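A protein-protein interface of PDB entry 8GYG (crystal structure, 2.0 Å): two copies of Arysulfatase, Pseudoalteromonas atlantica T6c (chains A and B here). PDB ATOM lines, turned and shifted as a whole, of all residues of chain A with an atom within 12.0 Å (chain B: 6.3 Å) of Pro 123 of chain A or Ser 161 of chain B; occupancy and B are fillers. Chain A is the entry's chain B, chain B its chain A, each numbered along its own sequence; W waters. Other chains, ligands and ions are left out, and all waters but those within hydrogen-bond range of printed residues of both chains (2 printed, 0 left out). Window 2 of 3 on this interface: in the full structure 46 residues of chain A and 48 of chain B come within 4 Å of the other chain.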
ATOM      1  N   ALA A 116      22.109  -9.598 -17.094  1.00  0.00           N
ATOM      2  CA  ALA A 116      23.072  -8.689 -16.480  1.00  0.00           C
ATOM      3  C   ALA A 116      22.597  -8.225 -15.110  1.00  0.00           C
ATOM      4  O   ALA A 116      23.399  -8.089 -14.177  1.00  0.00           O
ATOM      5  CB  ALA A 116      23.308  -7.481 -17.388  1.00  0.00           C
ATOM      6  N   ALA A 117      21.296  -7.959 -14.982  1.00  0.00           N
ATOM      7  CA  ALA A 117      20.719  -7.599 -13.690  1.00  0.00           C
ATOM      8  C   ALA A 117      20.829  -8.750 -12.699  1.00  0.00           C
ATOM      9  O   ALA A 117      21.274  -8.563 -11.560  1.00  0.00           O
ATOM     10  CB  ALA A 117      19.257  -7.179 -13.874  1.00  0.00           C
ATOM     11  N   GLY A 118      20.420  -9.949 -13.112  1.00  0.00           N
ATOM     12  CA  GLY A 118      20.579 -11.111 -12.257  1.00  0.00           C
ATOM     13  C   GLY A 118      22.028 -11.404 -11.932  1.00  0.00           C
ATOM     14  O   GLY A 118      22.337 -11.893 -10.839  1.00  0.00           O
ATOM     15  N   HIS A 119      22.936 -11.091 -12.861  1.00  0.00           N
ATOM     16  CA  HIS A 119      24.371 -11.288 -12.679  1.00  0.00           C
ATOM     17  C   HIS A 119      24.681 -12.636 -12.032  1.00  0.00           C
ATOM     18  O   HIS A 119      24.106 -13.652 -12.431  1.00  0.00           O
ATOM     19  CB  HIS A 119      24.973 -10.136 -11.871  1.00  0.00           C
ATOM     20  CG  HIS A 119      26.440  -9.946 -12.101  1.00  0.00           C
ATOM     21  ND1 HIS A 119      27.185  -8.989 -11.445  1.00  0.00           N
ATOM     22  CD2 HIS A 119      27.305 -10.596 -12.919  1.00  0.00           C
ATOM     23  CE1 HIS A 119      28.442  -9.059 -11.844  1.00  0.00           C
ATOM     24  NE2 HIS A 119      28.541 -10.021 -12.743  1.00  0.00           N
ATOM     25  N   TYR A 120      25.571 -12.669 -11.033  1.00  0.00           N
ATOM     26  CA  TYR A 120      26.006 -13.947 -10.476  1.00  0.00           C
ATOM     27  C   TYR A 120      25.131 -14.446  -9.327  1.00  0.00           C
ATOM     28  O   TYR A 120      25.391 -15.536  -8.803  1.00  0.00           O
ATOM     29  CB  TYR A 120      27.483 -13.868 -10.047  1.00  0.00           C
ATOM     30  CG  TYR A 120      28.403 -14.254 -11.194  1.00  0.00           C
ATOM     31  CD1 TYR A 120      27.931 -15.073 -12.219  1.00  0.00           C
ATOM     32  CD2 TYR A 120      29.720 -13.794 -11.277  1.00  0.00           C
ATOM     33  CE1 TYR A 120      28.726 -15.441 -13.289  1.00  0.00           C
ATOM     34  CE2 TYR A 120      30.538 -14.166 -12.365  1.00  0.00           C
ATOM     35  CZ  TYR A 120      30.021 -14.994 -13.368  1.00  0.00           C
ATOM     36  OH  TYR A 120      30.773 -15.395 -14.461  1.00  0.00           O
ATOM     37  N   GLY A 121      24.085 -13.705  -8.954  1.00  0.00           N
ATOM     38  CA  GLY A 121      23.115 -14.202  -7.988  1.00  0.00           C
ATOM     39  C   GLY A 121      23.560 -14.165  -6.539  1.00  0.00           C
ATOM     40  O   GLY A 121      23.161 -15.035  -5.753  1.00  0.00           O
ATOM     41  N   VAL A 122      24.364 -13.177  -6.162  1.00  0.00           N
ATOM     42  CA  VAL A 122      24.950 -13.053  -4.830  1.00  0.00           C
ATOM     43  C   VAL A 122      24.362 -11.812  -4.168  1.00  0.00           C
ATOM     44  O   VAL A 122      24.590 -10.694  -4.653  1.00  0.00           O
ATOM     45  CB  VAL A 122      26.484 -12.972  -4.903  1.00  0.00           C
ATOM     46  CG1 VAL A 122      27.076 -12.597  -3.542  1.00  0.00           C
ATOM     47  CG2 VAL A 122      27.072 -14.287  -5.406  1.00  0.00           C
ATOM     48  N   PRO A 123      23.617 -11.946  -3.065  1.00  0.00           N
ATOM     49  CA  PRO A 123      23.021 -10.760  -2.428  1.00  0.00           C
ATOM     50  C   PRO A 123      24.096  -9.749  -2.045  1.00  0.00           C
ATOM     51  O   PRO A 123      25.115 -10.095  -1.441  1.00  0.00           O
ATOM     52  CB  PRO A 123      22.317 -11.334  -1.186  1.00  0.00           C
ATOM     53  CG  PRO A 123      22.244 -12.809  -1.390  1.00  0.00           C
ATOM     54  CD  PRO A 123      23.413 -13.166  -2.263  1.00  0.00           C
ATOM     55  N   GLY A 124      23.874  -8.496  -2.427  1.00  0.00           N
ATOM     56  CA  GLY A 124      24.867  -7.456  -2.251  1.00  0.00           C
ATOM     57  C   GLY A 124      25.673  -7.126  -3.492  1.00  0.00           C
ATOM     58  O   GLY A 124      26.421  -6.136  -3.477  1.00  0.00           O
ATOM     59  N   GLN A 125      25.540  -7.915  -4.561  1.00  0.00           N
ATOM     60  CA  GLN A 125      26.208  -7.610  -5.823  1.00  0.00           C
ATOM     61  C   GLN A 125      25.866  -6.194  -6.284  1.00  0.00           C
ATOM     62  O   GLN A 125      24.748  -5.709  -6.088  1.00  0.00           O
ATOM     63  CB  GLN A 125      25.809  -8.640  -6.893  1.00  0.00           C
ATOM     64  CG  GLN A 125      24.303  -8.683  -7.247  1.00  0.00           C
ATOM     65  CD  GLN A 125      23.916  -9.919  -8.068  1.00  0.00           C
ATOM     66  OE1 GLN A 125      24.610 -10.941  -8.044  1.00  0.00           O
ATOM     67  NE2 GLN A 125      22.797  -9.826  -8.799  1.00  0.00           N
ATOM     68  N   ILE A 126      26.851  -5.521  -6.872  1.00  0.00           N
ATOM     69  CA  ILE A 126      26.680  -4.152  -7.361  1.00  0.00           C
ATOM     70  C   ILE A 126      26.139  -4.158  -8.788  1.00  0.00           C
ATOM     71  O   ILE A 126      26.728  -4.806  -9.668  1.00  0.00           O
ATOM     72  CB  ILE A 126      28.005  -3.373  -7.311  1.00  0.00           C
ATOM     73  CG1 ILE A 126      28.524  -3.280  -5.880  1.00  0.00           C
ATOM     74  CG2 ILE A 126      27.846  -1.993  -7.941  1.00  0.00           C
ATOM     75  CD1 ILE A 126      30.016  -3.064  -5.826  1.00  0.00           C
ATOM     76  N   PRO A 127      25.058  -3.431  -9.073  1.00  0.00           N
ATOM     77  CA  PRO A 127      24.576  -3.355 -10.459  1.00  0.00           C
ATOM     78  C   PRO A 127      25.547  -2.607 -11.369  1.00  0.00           C
ATOM     79  O   PRO A 127      26.127  -1.584 -10.998  1.00  0.00           O
ATOM     80  CB  PRO A 127      23.232  -2.618 -10.335  1.00  0.00           C
ATOM     81  CG  PRO A 127      23.305  -1.893  -9.028  1.00  0.00           C
ATOM     82  CD  PRO A 127      24.147  -2.762  -8.128  1.00  0.00           C
ATOM     83  N   THR B 158      20.952 -24.595  -7.161  1.00  0.00           N
ATOM     84  CA  THR B 158      21.685 -23.742  -6.233  1.00  0.00           C
ATOM     85  C   THR B 158      22.723 -22.849  -6.918  1.00  0.00           C
ATOM     86  O   THR B 158      23.639 -22.348  -6.248  1.00  0.00           O
ATOM     87  CB  THR B 158      22.347 -24.590  -5.155  1.00  0.00           C
ATOM     88  OG1 THR B 158      23.228 -25.550  -5.761  1.00  0.00           O
ATOM     89  CG2 THR B 158      21.276 -25.318  -4.339  1.00  0.00           C
ATOM     90  N   HIS B 159      22.590 -22.614  -8.227  1.00  0.00           N
ATOM     91  CA  HIS B 159      23.560 -21.764  -8.913  1.00  0.00           C
ATOM     92  C   HIS B 159      23.492 -20.330  -8.423  1.00  0.00           C
ATOM     93  O   HIS B 159      24.499 -19.612  -8.478  1.00  0.00           O
ATOM     94  CB  HIS B 159      23.352 -21.809 -10.423  1.00  0.00           C
ATOM     95  CG  HIS B 159      24.510 -21.272 -11.206  1.00  0.00           C
ATOM     96  ND1 HIS B 159      25.821 -21.580 -10.905  1.00  0.00           N
ATOM     97  CD2 HIS B 159      24.556 -20.455 -12.286  1.00  0.00           C
ATOM     98  CE1 HIS B 159      26.625 -20.968 -11.756  1.00  0.00           C
ATOM     99  NE2 HIS B 159      25.884 -20.278 -12.605  1.00  0.00           N
ATOM    100  N   PHE B 160      22.321 -19.890  -7.970  1.00  0.00           N
ATOM    101  CA  PHE B 160      22.143 -18.582  -7.369  1.00  0.00           C
ATOM    102  C   PHE B 160      21.901 -18.756  -5.876  1.00  0.00           C
ATOM    103  O   PHE B 160      21.505 -19.830  -5.405  1.00  0.00           O
ATOM    104  CB  PHE B 160      20.972 -17.823  -8.010  1.00  0.00           C
ATOM    105  CG  PHE B 160      21.121 -17.604  -9.494  1.00  0.00           C
ATOM    106  CD1 PHE B 160      22.373 -17.389 -10.060  1.00  0.00           C
ATOM    107  CD2 PHE B 160      20.010 -17.624 -10.323  1.00  0.00           C
ATOM    108  CE1 PHE B 160      22.516 -17.194 -11.431  1.00  0.00           C
ATOM    109  CE2 PHE B 160      20.139 -17.423 -11.693  1.00  0.00           C
ATOM    110  CZ  PHE B 160      21.398 -17.205 -12.249  1.00  0.00           C
ATOM    111  N   SER B 161      22.131 -17.677  -5.131  1.00  0.00           N
ATOM    112  CA  SER B 161      22.039 -17.698  -3.674  1.00  0.00           C
ATOM    113  C   SER B 161      21.007 -16.701  -3.164  1.00  0.00           C
ATOM    114  O   SER B 161      21.189 -16.088  -2.112  1.00  0.00           O
ATOM    115  CB  SER B 161      23.404 -17.413  -3.051  1.00  0.00           C
ATOM    116  OG  SER B 161      24.291 -18.503  -3.275  1.00  0.00           O
ATOM    117  N   TRP B 162      19.946 -16.505  -3.905  1.00  0.00           N
ATOM    118  CA  TRP B 162      18.956 -15.584  -3.379  1.00  0.00           C
ATOM    119  C   TRP B 162      18.170 -16.267  -2.264  1.00  0.00           C
ATOM    120  O   TRP B 162      17.875 -17.465  -2.359  1.00  0.00           O
ATOM    121  CB  TRP B 162      18.014 -15.128  -4.472  1.00  0.00           C
ATOM    122  CG  TRP B 162      18.694 -14.468  -5.621  1.00  0.00           C
ATOM    123  CD1 TRP B 162      18.735 -14.918  -6.905  1.00  0.00           C
ATOM    124  CD2 TRP B 162      19.412 -13.225  -5.606  1.00  0.00           C
ATOM    125  NE1 TRP B 162      19.429 -14.036  -7.693  1.00  0.00           N
ATOM    126  CE2 TRP B 162      19.858 -12.988  -6.921  1.00  0.00           C
ATOM    127  CE3 TRP B 162      19.722 -12.291  -4.608  1.00  0.00           C
ATOM    128  CZ2 TRP B 162      20.598 -11.860  -7.268  1.00  0.00           C
ATOM    129  CZ3 TRP B 162      20.459 -11.170  -4.951  1.00  0.00           C
ATOM    130  CH2 TRP B 162      20.894 -10.966  -6.270  1.00  0.00           C
ATOM    131  N   PRO B 163      17.860 -15.541  -1.190  1.00  0.00           N
ATOM    132  CA  PRO B 163      17.097 -16.138  -0.087  1.00  0.00           C
ATOM    133  C   PRO B 163      15.724 -16.580  -0.563  1.00  0.00           C
ATOM    134  O   PRO B 163      14.993 -15.823  -1.208  1.00  0.00           O
ATOM    135  CB  PRO B 163      17.007 -15.002   0.939  1.00  0.00           C
ATOM    136  CG  PRO B 163      18.161 -14.110   0.626  1.00  0.00           C
ATOM    137  CD  PRO B 163      18.323 -14.178  -0.870  1.00  0.00           C
ATOM    138  N   THR B 243      30.436 -22.369  -4.025  1.00  0.00           N
ATOM    139  CA  THR B 243      29.021 -22.413  -3.690  1.00  0.00           C
ATOM    140  C   THR B 243      28.156 -22.665  -4.922  1.00  0.00           C
ATOM    141  O   THR B 243      27.078 -23.261  -4.814  1.00  0.00           O
ATOM    142  CB  THR B 243      28.625 -21.091  -3.016  1.00  0.00           C
ATOM    143  OG1 THR B 243      29.436 -20.897  -1.842  1.00  0.00           O
ATOM    144  CG2 THR B 243      27.166 -21.088  -2.611  1.00  0.00           C
ATOM    145  N   HIS B 244      28.626 -22.252  -6.097  1.00  0.00           N
ATOM    146  CA  HIS B 244      27.768 -22.130  -7.264  1.00  0.00           C
ATOM    147  C   HIS B 244      28.145 -23.090  -8.377  1.00  0.00           C
ATOM    148  O   HIS B 244      27.560 -23.012  -9.465  1.00  0.00           O
ATOM    149  CB  HIS B 244      27.793 -20.685  -7.773  1.00  0.00           C
ATOM    150  CG  HIS B 244      27.119 -19.718  -6.857  1.00  0.00           C
ATOM    151  ND1 HIS B 244      27.359 -18.360  -6.897  1.00  0.00           N
ATOM    152  CD2 HIS B 244      26.203 -19.912  -5.876  1.00  0.00           C
ATOM    153  CE1 HIS B 244      26.619 -17.760  -5.980  1.00  0.00           C
ATOM    154  NE2 HIS B 244      25.912 -18.679  -5.346  1.00  0.00           N
HETATM  155  O   HOH W   1      26.240 -17.842 -10.166  1.00  0.00           O
HETATM  156  O   HOH W   2      20.593 -14.107 -10.424  1.00  0.00           O
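Water W1 lies within hydrogen-bond range of the backbone carbonyl oxygen (O) of Tyr 120 of chain A (2.8 Å), the backbone carbonyl oxygen (O) of His 159 of chain B (3.0 Å) and a ring nitrogen (ND1) of His 244 of chain B (3.5 Å). Water W2 bridges O of Gly 118 of chain A and NE1 of Trp 162 of chain B.
N of Ser 161 of chain B lies within hydrogen-bond range of O of Gly 121 of chain A, at 2.9 Å.
Of chain B, only Ser 161 (3.5 Å) and Trp 162 (3.6 Å) come within 4 Å of Pro 123 of chain A. Ser 161 of chain B touches just these residues of chain A: Gly 121 and Pro 123. No residue of chain A comes within 4 Å of Thr 158 of chain B. Of chain A, only Gly 118, Gly 121, Pro 123 and Gln 125 come within 4 Å of Trp 162 of chain B. Pro 163 of chain B touches none of the printed residues of chain A. No residue of chain A comes within 4 Å of Thr 243 of chain B. Of the printed residues of chain B, Gly 118 of chain A touches Trp 162 (3.97 Å). Printed residues of chain B within 4 Å of Gln 125 of chain A: Trp 162. Of the printed residues of chain A, Phe 160 of chain B touches Tyr 120 and Gly 121. Of the printed residues of chain A, His 244 of chain B touches Tyr 120 (3.8 Å) and Val 122 (3.5 Å). Of the printed residues of chain B, Val 122 of chain A touches His 244 (3.5 Å). Gly 124 of chain A touches none of the printed residues of chain B. The nearest residue of chain B that does not touch Pro 123 of chain A is Pro 163 of chain B (4.2 Å).
Among the printed residues, merely in contact across the chains: Gly 118 of chain A with Trp 162 of chain B (3.97 Å), Tyr 120 of chain A with Phe 160 of chain B (3.8 Å), Tyr 120 of chain A with His 244 of chain B (3.8 Å), Gly 121 of chain A with Phe 160 of chain B (3.9 Å), Gly 121 of chain A with Trp 162 of chain B (3.5 Å), Val 122 of chain A with His 244 of chain B (3.5 Å), Pro 123 of chain A with Ser 161 of chain B (3.5 Å), Pro 123 of chain A with Trp 162 of chain B (3.6 Å) and Gln 125 of chain A with Trp 162 of chain B (3.4 Å).
Hydrophobic or aromatic side chains of chain A that line the printed part of chain B: Val 122 and Pro 123. Of the 8 printed residues of chain B, 4 touch a printed residue of chain A. Hydrophobic or aromatic side chains of chain B within 4 Å of the printed part of chain A: Phe 160, Trp 162 and His 244. Among the printed residues, no Asp or Glu carboxylate lies within 4 Å of a Lys or Arg side-chain nitrogen of the other chain.
The backbone carbonyl oxygen (O) of Gly 118 of chain A lies within hydrogen-bond range of the side-chain amide nitrogen (NE2) of Gln 125 of chain A, 2.9 Å away. O of His 244 of chain B lies within hydrogen-bond range of ND1 of His 159 of chain B (2.7 Å). The backbone NH (N) of Gly 121 of chain A sits at hydrogen-bond distance from the side-chain amide oxygen (OE1) of Gln 125 of chain A, 3.0 Å away. OG of Ser 161 of chain B sits at hydrogen-bond distance from NE2 of His 244 of chain B, at 2.6 Å. The backbone carbonyl oxygen (O) of Ala 117 of chain A lies within hydrogen-bond range of the side-chain amide nitrogen (NE2) of Gln 125 of chain A, at 3.4 Å. The backbone NH (N) of Val 122 of chain A is in hydrogen-bond range of the side-chain amide oxygen (OE1) of Gln 125 of chain A (2.9 Å).
No position is printed for both chains. Of the 10 pairs that touch across the chains among the printed residues, none has its exchanged pair printed and touching as well.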
